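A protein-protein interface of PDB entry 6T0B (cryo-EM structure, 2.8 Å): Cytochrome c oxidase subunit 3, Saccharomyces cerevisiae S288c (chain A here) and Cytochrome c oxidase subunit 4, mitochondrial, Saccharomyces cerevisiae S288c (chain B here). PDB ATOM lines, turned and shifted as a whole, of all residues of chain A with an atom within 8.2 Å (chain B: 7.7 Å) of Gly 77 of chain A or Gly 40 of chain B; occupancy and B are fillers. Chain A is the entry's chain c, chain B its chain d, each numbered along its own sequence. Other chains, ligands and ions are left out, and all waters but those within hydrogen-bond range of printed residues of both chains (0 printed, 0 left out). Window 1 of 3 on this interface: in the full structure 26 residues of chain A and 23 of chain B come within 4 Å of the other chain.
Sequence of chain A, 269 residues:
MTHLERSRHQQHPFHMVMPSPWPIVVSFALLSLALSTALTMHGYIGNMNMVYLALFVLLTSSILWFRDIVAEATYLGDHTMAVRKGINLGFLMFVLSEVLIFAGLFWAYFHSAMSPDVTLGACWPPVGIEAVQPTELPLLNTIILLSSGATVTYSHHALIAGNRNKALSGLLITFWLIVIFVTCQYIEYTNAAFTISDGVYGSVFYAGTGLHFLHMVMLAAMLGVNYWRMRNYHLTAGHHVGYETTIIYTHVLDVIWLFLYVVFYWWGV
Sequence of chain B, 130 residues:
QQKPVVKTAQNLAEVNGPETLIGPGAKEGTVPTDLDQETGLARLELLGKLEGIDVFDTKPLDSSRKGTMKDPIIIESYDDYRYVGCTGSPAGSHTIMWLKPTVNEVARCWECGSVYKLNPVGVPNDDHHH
Hydrophobic or aromatic side chains of chain B that line the printed part of chain A: Leu 41, Ala 42 and Leu 44.
Of the 16 printed residues of chain A, 7 touch a printed residue of chain B.
Hydrophobic or aromatic side chains of chain A that line the printed part of chain B: His 9 and His 239.
Among the printed residues, no Asp or Glu carboxylate lies within 4 Å of a Lys or Arg side-chain nitrogen of the other chain.
Printed residues of chain B within 4 Å of His 9 of chain A: Gly 17 and Leu 44.
Printed residues of chain B within 4 Å of Leu 76 of chain A: Thr 39 (3.5 Å) and Gly 40 (3.99 Å).
Gly 77 of chain A touches four residues of chain B.
Of the printed residues of chain B, His 239 of chain A touches Glu 38.
Of the printed residues of chain A, Glu 38 of chain B touches His 239 (2.9 Å).
Of chain A, only Leu 76 (3.5 Å) and Gly 77 (3.3 Å) come within 4 Å of Thr 39 of chain B.
Printed residues of chain A within 4 Å of Gly 40 of chain B: Leu 76 (3.99 Å) and Gly 77 (3.8 Å).
Of the printed residues of chain A, Leu 41 of chain B touches Gln 10 (3.2 Å), Gly 77 (3.2 Å) and Thr 80 (3.8 Å).
The nearest residue of chain B that does not touch Gly 77 of chain A is Glu 38 of chain B (4.2 Å).
The backbone carbonyl oxygen (O) of Gly 77 of chain A sits at hydrogen-bond distance from the backbone NH (N) of Leu 41 of chain B (3.2 Å).
The side-chain hydroxyl (OG1) of Thr 39 of chain B lies within hydrogen-bond range of the backbone NH (N) of Gly 77 of chain A.
The backbone carbonyl oxygen of Gly 77 of chain A lies within hydrogen-bond range of the backbone NH of Ala 42 of chain B (3.4 Å).
A ring nitrogen (ND1) of His 239 of chain A lies within hydrogen-bond range of the side-chain carboxylate (OE1) of Glu 38 of chain B.
His 9 of chain A touches Gly 17 of chain B.
CD2 of Leu 44 of chain B touches CD2 of His 9 of chain A, at 3.5 Å.
Gln 10 of chain A touches Leu 41 of chain B.
Leu 76 of chain A touches Thr 39 of chain B.
Leu 76 of chain A touches Gly 40 of chain B (O to CA, 3.99 Å).
O of Gly 77 of chain A touches C of Gly 40 of chain B, at 3.8 Å.
His 79 of chain A touches Ala 42 of chain B.
Leu 41 of chain B touches Thr 80 of chain A.
Thr 80 of chain A touches Glu 45 of chain B.
O of Ala 71 of chain A sits at hydrogen-bond distance from N of Leu 76 of chain A.
NH1 of Arg 43 of chain B sits at hydrogen-bond distance from O of Glu 38 of chain B (2.9 Å).
N of Gly 77 of chain A is in hydrogen-bond range of O of Glu 72 of chain A (3.4 Å).
O of Pro 13 of chain A lies within hydrogen-bond range of OG1 of Thr 80 of chain A (2.7 Å).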
ATOM      1  N   HIS A   9     -29.633  18.830  18.996  1.00  0.00           N
ATOM      2  CA  HIS A   9     -28.866  19.975  18.538  1.00  0.00           C
ATOM      3  C   HIS A   9     -29.769  20.794  17.630  1.00  0.00           C
ATOM      4  O   HIS A   9     -30.979  20.572  17.571  1.00  0.00           O
ATOM      5  CB  HIS A   9     -27.574  19.526  17.856  1.00  0.00           C
ATOM      6  CG  HIS A   9     -26.613  18.832  18.770  1.00  0.00           C
ATOM      7  ND1 HIS A   9     -26.704  17.494  19.069  1.00  0.00           N
ATOM      8  CD2 HIS A   9     -25.532  19.290  19.438  1.00  0.00           C
ATOM      9  CE1 HIS A   9     -25.721  17.155  19.881  1.00  0.00           C
ATOM     10  NE2 HIS A   9     -24.999  18.228  20.124  1.00  0.00           N
ATOM     11  N   GLN A  10     -29.194  21.735  16.892  1.00  0.00           N
ATOM     12  CA  GLN A  10     -29.997  22.860  16.437  1.00  0.00           C
ATOM     13  C   GLN A  10     -30.632  22.696  15.063  1.00  0.00           C
ATOM     14  O   GLN A  10     -31.560  23.453  14.757  1.00  0.00           O
ATOM     15  CB  GLN A  10     -29.165  24.140  16.438  1.00  0.00           C
ATOM     16  CG  GLN A  10     -29.955  25.322  16.925  1.00  0.00           C
ATOM     17  CD  GLN A  10     -29.207  26.605  16.829  1.00  0.00           C
ATOM     18  OE1 GLN A  10     -27.990  26.619  16.827  1.00  0.00           O
ATOM     19  NE2 GLN A  10     -29.929  27.703  16.756  1.00  0.00           N
ATOM     20  N   PRO A  13     -27.475  26.242  11.209  1.00  0.00           N
ATOM     21  CA  PRO A  13     -26.195  26.697  11.756  1.00  0.00           C
ATOM     22  C   PRO A  13     -26.214  28.046  12.439  1.00  0.00           C
ATOM     23  O   PRO A  13     -25.147  28.619  12.656  1.00  0.00           O
ATOM     24  CB  PRO A  13     -25.298  26.767  10.516  1.00  0.00           C
ATOM     25  CG  PRO A  13     -26.071  26.153   9.425  1.00  0.00           C
ATOM     26  CD  PRO A  13     -27.480  26.343   9.750  1.00  0.00           C
ATOM     27  N   HIS A  15     -27.107  31.322  15.062  1.00  0.00           N
ATOM     28  CA  HIS A  15     -27.031  31.646  16.479  1.00  0.00           C
ATOM     29  C   HIS A  15     -28.359  32.205  16.949  1.00  0.00           C
ATOM     30  O   HIS A  15     -28.746  33.308  16.560  1.00  0.00           O
ATOM     31  CB  HIS A  15     -25.918  32.656  16.725  1.00  0.00           C
ATOM     32  CG  HIS A  15     -25.619  32.887  18.168  1.00  0.00           C
ATOM     33  ND1 HIS A  15     -25.043  34.046  18.630  1.00  0.00           N
ATOM     34  CD2 HIS A  15     -25.811  32.103  19.252  1.00  0.00           C
ATOM     35  CE1 HIS A  15     -24.893  33.967  19.938  1.00  0.00           C
ATOM     36  NE2 HIS A  15     -25.345  32.795  20.339  1.00  0.00           N
ATOM     37  N   VAL A  70     -17.871  38.016  23.185  1.00  0.00           N
ATOM     38  CA  VAL A  70     -16.676  37.200  23.378  1.00  0.00           C
ATOM     39  C   VAL A  70     -17.024  35.907  24.097  1.00  0.00           C
ATOM     40  O   VAL A  70     -16.545  34.826  23.730  1.00  0.00           O
ATOM     41  CB  VAL A  70     -15.613  38.017  24.135  1.00  0.00           C
ATOM     42  CG1 VAL A  70     -14.576  37.133  24.783  1.00  0.00           C
ATOM     43  CG2 VAL A  70     -14.966  38.995  23.195  1.00  0.00           C
ATOM     44  N   ALA A  71     -17.919  35.989  25.081  1.00  0.00           N
ATOM     45  CA  ALA A  71     -18.352  34.812  25.824  1.00  0.00           C
ATOM     46  C   ALA A  71     -19.103  33.832  24.941  1.00  0.00           C
ATOM     47  O   ALA A  71     -18.884  32.625  25.035  1.00  0.00           O
ATOM     48  CB  ALA A  71     -19.228  35.238  26.993  1.00  0.00           C
ATOM     49  N   GLU A  72     -19.972  34.337  24.067  1.00  0.00           N
ATOM     50  CA  GLU A  72     -20.689  33.474  23.134  1.00  0.00           C
ATOM     51  C   GLU A  72     -19.748  32.831  22.135  1.00  0.00           C
ATOM     52  O   GLU A  72     -19.919  31.666  21.778  1.00  0.00           O
ATOM     53  CB  GLU A  72     -21.743  34.267  22.377  1.00  0.00           C
ATOM     54  CG  GLU A  72     -22.903  34.736  23.182  1.00  0.00           C
ATOM     55  CD  GLU A  72     -23.539  35.943  22.565  1.00  0.00           C
ATOM     56  OE1 GLU A  72     -23.180  36.261  21.419  1.00  0.00           O
ATOM     57  OE2 GLU A  72     -24.392  36.579  23.209  1.00  0.00           O
ATOM     58  N   ALA A  73     -18.760  33.572  21.666  1.00  0.00           N
ATOM     59  CA  ALA A  73     -17.914  33.053  20.610  1.00  0.00           C
ATOM     60  C   ALA A  73     -16.868  32.098  21.139  1.00  0.00           C
ATOM     61  O   ALA A  73     -16.401  31.232  20.396  1.00  0.00           O
ATOM     62  CB  ALA A  73     -17.231  34.198  19.873  1.00  0.00           C
ATOM     63  N   THR A  74     -16.470  32.237  22.392  1.00  0.00           N
ATOM     64  CA  THR A  74     -15.374  31.437  22.906  1.00  0.00           C
ATOM     65  C   THR A  74     -15.808  30.379  23.902  1.00  0.00           C
ATOM     66  O   THR A  74     -15.366  29.234  23.812  1.00  0.00           O
ATOM     67  CB  THR A  74     -14.333  32.350  23.549  1.00  0.00           C
ATOM     68  OG1 THR A  74     -13.919  33.324  22.595  1.00  0.00           O
ATOM     69  CG2 THR A  74     -13.143  31.576  23.941  1.00  0.00           C
ATOM     70  N   TYR A  75     -16.701  30.709  24.822  1.00  0.00           N
ATOM     71  CA  TYR A  75     -17.024  29.812  25.910  1.00  0.00           C
ATOM     72  C   TYR A  75     -18.317  29.045  25.710  1.00  0.00           C
ATOM     73  O   TYR A  75     -18.652  28.211  26.550  1.00  0.00           O
ATOM     74  CB  TYR A  75     -17.101  30.589  27.211  1.00  0.00           C
ATOM     75  CG  TYR A  75     -15.880  31.407  27.476  1.00  0.00           C
ATOM     76  CD1 TYR A  75     -14.632  30.840  27.436  1.00  0.00           C
ATOM     77  CD2 TYR A  75     -15.979  32.750  27.759  1.00  0.00           C
ATOM     78  CE1 TYR A  75     -13.520  31.587  27.673  1.00  0.00           C
ATOM     79  CE2 TYR A  75     -14.878  33.501  27.994  1.00  0.00           C
ATOM     80  CZ  TYR A  75     -13.652  32.915  27.957  1.00  0.00           C
ATOM     81  OH  TYR A  75     -12.541  33.676  28.194  1.00  0.00           O
ATOM     82  N   LEU A  76     -19.057  29.306  24.645  1.00  0.00           N
ATOM     83  CA  LEU A  76     -20.255  28.544  24.346  1.00  0.00           C
ATOM     84  C   LEU A  76     -20.235  27.910  22.974  1.00  0.00           C
ATOM     85  O   LEU A  76     -21.057  27.030  22.717  1.00  0.00           O
ATOM     86  CB  LEU A  76     -21.506  29.423  24.457  1.00  0.00           C
ATOM     87  CG  LEU A  76     -21.752  30.087  25.804  1.00  0.00           C
ATOM     88  CD1 LEU A  76     -22.979  30.945  25.730  1.00  0.00           C
ATOM     89  CD2 LEU A  76     -21.909  29.040  26.867  1.00  0.00           C
ATOM     90  N   GLY A  77     -19.328  28.316  22.101  1.00  0.00           N
ATOM     91  CA  GLY A  77     -19.166  27.707  20.805  1.00  0.00           C
ATOM     92  C   GLY A  77     -20.353  27.920  19.905  1.00  0.00           C
ATOM     93  O   GLY A  77     -20.900  26.967  19.353  1.00  0.00           O
ATOM     94  N   ASP A  78     -20.764  29.164  19.753  1.00  0.00           N
ATOM     95  CA  ASP A  78     -21.982  29.483  19.039  1.00  0.00           C
ATOM     96  C   ASP A  78     -21.732  30.063  17.666  1.00  0.00           C
ATOM     97  O   ASP A  78     -22.692  30.344  16.951  1.00  0.00           O
ATOM     98  CB  ASP A  78     -22.811  30.468  19.847  1.00  0.00           C
ATOM     99  CG  ASP A  78     -23.806  29.788  20.742  1.00  0.00           C
ATOM    100  OD1 ASP A  78     -23.970  28.561  20.615  1.00  0.00           O
ATOM    101  OD2 ASP A  78     -24.427  30.478  21.572  1.00  0.00           O
ATOM    102  N   HIS A  79     -20.485  30.253  17.278  1.00  0.00           N
ATOM    103  CA  HIS A  79     -20.157  30.894  16.011  1.00  0.00           C
ATOM    104  C   HIS A  79     -19.695  29.818  15.040  1.00  0.00           C
ATOM    105  O   HIS A  79     -18.525  29.444  15.013  1.00  0.00           O
ATOM    106  CB  HIS A  79     -19.107  31.959  16.199  1.00  0.00           C
ATOM    107  CG  HIS A  79     -19.623  33.201  16.847  1.00  0.00           C
ATOM    108  ND1 HIS A  79     -19.055  34.435  16.643  1.00  0.00           N
ATOM    109  CD2 HIS A  79     -20.651  33.397  17.704  1.00  0.00           C
ATOM    110  CE1 HIS A  79     -19.712  35.339  17.343  1.00  0.00           C
ATOM    111  NE2 HIS A  79     -20.689  34.736  17.991  1.00  0.00           N
ATOM    112  N   THR A  80     -20.625  29.338  14.230  1.00  0.00           N
ATOM    113  CA  THR A  80     -20.345  28.337  13.216  1.00  0.00           C
ATOM    114  C   THR A  80     -19.839  29.033  11.956  1.00  0.00           C
ATOM    115  O   THR A  80     -19.519  30.223  11.973  1.00  0.00           O
ATOM    116  CB  THR A  80     -21.592  27.518  12.956  1.00  0.00           C
ATOM    117  OG1 THR A  80     -22.511  28.304  12.199  1.00  0.00           O
ATOM    118  CG2 THR A  80     -22.241  27.146  14.249  1.00  0.00           C
ATOM    119  N   HIS A 239     -10.050  30.222  13.570  1.00  0.00           N
ATOM    120  CA  HIS A 239     -11.274  30.895  13.979  1.00  0.00           C
ATOM    121  C   HIS A 239     -10.866  32.167  14.708  1.00  0.00           C
ATOM    122  O   HIS A 239     -10.766  32.188  15.933  1.00  0.00           O
ATOM    123  CB  HIS A 239     -12.099  29.965  14.840  1.00  0.00           C
ATOM    124  CG  HIS A 239     -13.450  30.490  15.179  1.00  0.00           C
ATOM    125  ND1 HIS A 239     -14.227  29.946  16.175  1.00  0.00           N
ATOM    126  CD2 HIS A 239     -14.163  31.512  14.659  1.00  0.00           C
ATOM    127  CE1 HIS A 239     -15.362  30.613  16.254  1.00  0.00           C
ATOM    128  NE2 HIS A 239     -15.350  31.566  15.343  1.00  0.00           N
ATOM    129  N   VAL B  15     -20.099  11.673  19.928  1.00  0.00           N
ATOM    130  CA  VAL B  15     -20.804  12.829  20.455  1.00  0.00           C
ATOM    131  C   VAL B  15     -22.021  12.335  21.218  1.00  0.00           C
ATOM    132  O   VAL B  15     -22.862  11.609  20.680  1.00  0.00           O
ATOM    133  CB  VAL B  15     -21.191  13.801  19.339  1.00  0.00           C
ATOM    134  CG1 VAL B  15     -21.945  14.965  19.907  1.00  0.00           C
ATOM    135  CG2 VAL B  15     -19.956  14.298  18.650  1.00  0.00           C
ATOM    136  N   GLY B  17     -24.444  14.400  23.518  1.00  0.00           N
ATOM    137  CA  GLY B  17     -24.860  15.641  24.114  1.00  0.00           C
ATOM    138  C   GLY B  17     -23.838  16.735  23.917  1.00  0.00           C
ATOM    139  O   GLY B  17     -22.952  16.629  23.073  1.00  0.00           O
ATOM    140  N   PRO B  18     -23.962  17.824  24.673  1.00  0.00           N
ATOM    141  CA  PRO B  18     -23.015  18.937  24.556  1.00  0.00           C
ATOM    142  C   PRO B  18     -21.888  18.959  25.576  1.00  0.00           C
ATOM    143  O   PRO B  18     -21.011  19.820  25.464  1.00  0.00           O
ATOM    144  CB  PRO B  18     -23.931  20.138  24.757  1.00  0.00           C
ATOM    145  CG  PRO B  18     -24.869  19.661  25.773  1.00  0.00           C
ATOM    146  CD  PRO B  18     -25.141  18.217  25.455  1.00  0.00           C
ATOM    147  N   THR B  20     -19.686  16.702  25.755  1.00  0.00           N
ATOM    148  CA  THR B  20     -18.649  15.905  25.142  1.00  0.00           C
ATOM    149  C   THR B  20     -17.878  16.687  24.103  1.00  0.00           C
ATOM    150  O   THR B  20     -16.937  16.158  23.511  1.00  0.00           O
ATOM    151  CB  THR B  20     -19.269  14.688  24.494  1.00  0.00           C
ATOM    152  OG1 THR B  20     -18.235  13.787  24.105  1.00  0.00           O
ATOM    153  CG2 THR B  20     -20.027  15.122  23.283  1.00  0.00           C
ATOM    154  N   LEU B  21     -18.265  17.933  23.862  1.00  0.00           N
ATOM    155  CA  LEU B  21     -17.659  18.753  22.825  1.00  0.00           C
ATOM    156  C   LEU B  21     -16.747  19.804  23.413  1.00  0.00           C
ATOM    157  O   LEU B  21     -16.752  20.932  22.949  1.00  0.00           O
ATOM    158  CB  LEU B  21     -18.739  19.413  21.981  1.00  0.00           C
ATOM    159  CG  LEU B  21     -19.706  18.524  21.210  1.00  0.00           C
ATOM    160  CD1 LEU B  21     -21.043  19.194  21.122  1.00  0.00           C
ATOM    161  CD2 LEU B  21     -19.192  18.240  19.830  1.00  0.00           C
ATOM    162  N   ILE B  22     -15.968  19.491  24.440  1.00  0.00           N
ATOM    163  CA  ILE B  22     -15.265  20.542  25.156  1.00  0.00           C
ATOM    164  C   ILE B  22     -13.902  20.816  24.536  1.00  0.00           C
ATOM    165  O   ILE B  22     -13.653  21.915  24.032  1.00  0.00           O
ATOM    166  CB  ILE B  22     -15.153  20.203  26.648  1.00  0.00           C
ATOM    167  CG1 ILE B  22     -16.533  20.258  27.283  1.00  0.00           C
ATOM    168  CG2 ILE B  22     -14.275  21.201  27.358  1.00  0.00           C
ATOM    169  CD1 ILE B  22     -17.178  21.609  27.207  1.00  0.00           C
ATOM    170  N   GLN B  37      -9.539  24.078  21.035  1.00  0.00           N
ATOM    171  CA  GLN B  37     -10.411  24.944  21.809  1.00  0.00           C
ATOM    172  C   GLN B  37     -11.658  25.410  21.076  1.00  0.00           C
ATOM    173  O   GLN B  37     -11.973  26.602  21.091  1.00  0.00           O
ATOM    174  CB  GLN B  37      -9.635  26.163  22.272  1.00  0.00           C
ATOM    175  CG  GLN B  37      -8.507  25.843  23.188  1.00  0.00           C
ATOM    176  CD  GLN B  37      -7.704  27.050  23.477  1.00  0.00           C
ATOM    177  OE1 GLN B  37      -8.088  28.148  23.103  1.00  0.00           O
ATOM    178  NE2 GLN B  37      -6.587  26.876  24.161  1.00  0.00           N
ATOM    179  N   GLU B  38     -12.374  24.502  20.436  1.00  0.00           N
ATOM    180  CA  GLU B  38     -13.689  24.808  19.902  1.00  0.00           C
ATOM    181  C   GLU B  38     -14.706  24.002  20.681  1.00  0.00           C
ATOM    182  O   GLU B  38     -14.405  22.901  21.132  1.00  0.00           O
ATOM    183  CB  GLU B  38     -13.784  24.484  18.421  1.00  0.00           C
ATOM    184  CG  GLU B  38     -14.969  25.096  17.717  1.00  0.00           C
ATOM    185  CD  GLU B  38     -14.939  26.609  17.723  1.00  0.00           C
ATOM    186  OE1 GLU B  38     -14.065  27.192  17.050  1.00  0.00           O
ATOM    187  OE2 GLU B  38     -15.790  27.219  18.404  1.00  0.00           O
ATOM    188  N   THR B  39     -15.888  24.565  20.895  1.00  0.00           N
ATOM    189  CA  THR B  39     -16.959  23.834  21.546  1.00  0.00           C
ATOM    190  C   THR B  39     -18.257  23.979  20.789  1.00  0.00           C
ATOM    191  O   THR B  39     -18.355  24.695  19.792  1.00  0.00           O
ATOM    192  CB  THR B  39     -17.231  24.289  22.968  1.00  0.00           C
ATOM    193  OG1 THR B  39     -17.547  25.680  22.966  1.00  0.00           O
ATOM    194  CG2 THR B  39     -16.088  24.034  23.836  1.00  0.00           C
ATOM    195  N   GLY B  40     -19.247  23.262  21.307  1.00  0.00           N
ATOM    196  CA  GLY B  40     -20.626  23.482  20.950  1.00  0.00           C
ATOM    197  C   GLY B  40     -20.929  23.129  19.515  1.00  0.00           C
ATOM    198  O   GLY B  40     -20.404  22.164  18.945  1.00  0.00           O
ATOM    199  N   LEU B  41     -21.788  23.949  18.925  1.00  0.00           N
ATOM    200  CA  LEU B  41     -22.248  23.709  17.571  1.00  0.00           C
ATOM    201  C   LEU B  41     -21.131  23.913  16.559  1.00  0.00           C
ATOM    202  O   LEU B  41     -21.079  23.209  15.541  1.00  0.00           O
ATOM    203  CB  LEU B  41     -23.424  24.624  17.278  1.00  0.00           C
ATOM    204  CG  LEU B  41     -24.186  24.262  16.024  1.00  0.00           C
ATOM    205  CD1 LEU B  41     -24.819  22.901  16.178  1.00  0.00           C
ATOM    206  CD2 LEU B  41     -25.228  25.296  15.779  1.00  0.00           C
ATOM    207  N   ALA B  42     -20.204  24.826  16.847  1.00  0.00           N
ATOM    208  CA  ALA B  42     -19.052  25.016  15.981  1.00  0.00           C
ATOM    209  C   ALA B  42     -18.136  23.805  16.000  1.00  0.00           C
ATOM    210  O   ALA B  42     -17.595  23.418  14.958  1.00  0.00           O
ATOM    211  CB  ALA B  42     -18.297  26.270  16.386  1.00  0.00           C
ATOM    212  N   ARG B  43     -17.985  23.157  17.155  1.00  0.00           N
ATOM    213  CA  ARG B  43     -17.181  21.943  17.184  1.00  0.00           C
ATOM    214  C   ARG B  43     -17.891  20.786  16.509  1.00  0.00           C
ATOM    215  O   ARG B  43     -17.236  19.941  15.891  1.00  0.00           O
ATOM    216  CB  ARG B  43     -16.817  21.558  18.608  1.00  0.00           C
ATOM    217  CG  ARG B  43     -15.671  20.582  18.639  1.00  0.00           C
ATOM    218  CD  ARG B  43     -15.358  20.028  19.983  1.00  0.00           C
ATOM    219  NE  ARG B  43     -14.215  19.140  19.882  1.00  0.00           N
ATOM    220  CZ  ARG B  43     -12.959  19.531  20.015  1.00  0.00           C
ATOM    221  NH1 ARG B  43     -12.683  20.792  20.266  1.00  0.00           N
ATOM    222  NH2 ARG B  43     -11.980  18.658  19.899  1.00  0.00           N
ATOM    223  N   LEU B  44     -19.218  20.738  16.608  1.00  0.00           N
ATOM    224  CA  LEU B  44     -19.977  19.702  15.917  1.00  0.00           C
ATOM    225  C   LEU B  44     -19.809  19.816  14.414  1.00  0.00           C
ATOM    226  O   LEU B  44     -19.553  18.821  13.724  1.00  0.00           O
ATOM    227  CB  LEU B  44     -21.443  19.816  16.295  1.00  0.00           C
ATOM    228  CG  LEU B  44     -22.294  18.589  16.054  1.00  0.00           C
ATOM    229  CD1 LEU B  44     -21.779  17.431  16.858  1.00  0.00           C
ATOM    230  CD2 LEU B  44     -23.701  18.910  16.437  1.00  0.00           C
ATOM    231  N   GLU B  45     -19.912  21.040  13.903  1.00  0.00           N
ATOM    232  CA  GLU B  45     -19.734  21.292  12.480  1.00  0.00           C
ATOM    233  C   GLU B  45     -18.306  21.003  12.036  1.00  0.00           C
ATOM    234  O   GLU B  45     -18.087  20.445  10.955  1.00  0.00           O
ATOM    235  CB  GLU B  45     -20.118  22.733  12.186  1.00  0.00           C
ATOM    236  CG  GLU B  45     -19.974  23.144  10.755  1.00  0.00           C
ATOM    237  CD  GLU B  45     -19.994  24.635  10.598  1.00  0.00           C
ATOM    238  OE1 GLU B  45     -20.935  25.153   9.970  1.00  0.00           O
ATOM    239  OE2 GLU B  45     -19.073  25.292  11.115  1.00  0.00           O
ATOM    240  N   LEU B  46     -17.327  21.335  12.880  1.00  0.00           N
ATOM    241  CA  LEU B  46     -15.930  21.054  12.570  1.00  0.00           C
ATOM    242  C   LEU B  46     -15.656  19.558  12.504  1.00  0.00           C
ATOM    243  O   LEU B  46     -14.953  19.094  11.598  1.00  0.00           O
ATOM    244  CB  LEU B  46     -15.044  21.716  13.615  1.00  0.00           C
ATOM    245  CG  LEU B  46     -13.613  21.236  13.737  1.00  0.00           C
ATOM    246  CD1 LEU B  46     -12.798  21.811  12.612  1.00  0.00           C
ATOM    247  CD2 LEU B  46     -13.055  21.646  15.073  1.00  0.00           C
ATOM    248  N   LEU B  47     -16.214  18.791  13.448  1.00  0.00           N
ATOM    249  CA  LEU B  47     -16.079  17.336  13.435  1.00  0.00           C
ATOM    250  C   LEU B  47     -16.704  16.731  12.191  1.00  0.00           C
ATOM    251  O   LEU B  47     -16.128  15.828  11.566  1.00  0.00           O
ATOM    252  CB  LEU B  47     -16.743  16.743  14.670  1.00  0.00           C
ATOM    253  CG  LEU B  47     -15.956  16.788  15.954  1.00  0.00           C
ATOM    254  CD1 LEU B  47     -16.736  16.080  17.014  1.00  0.00           C
ATOM    255  CD2 LEU B  47     -14.642  16.115  15.729  1.00  0.00           C
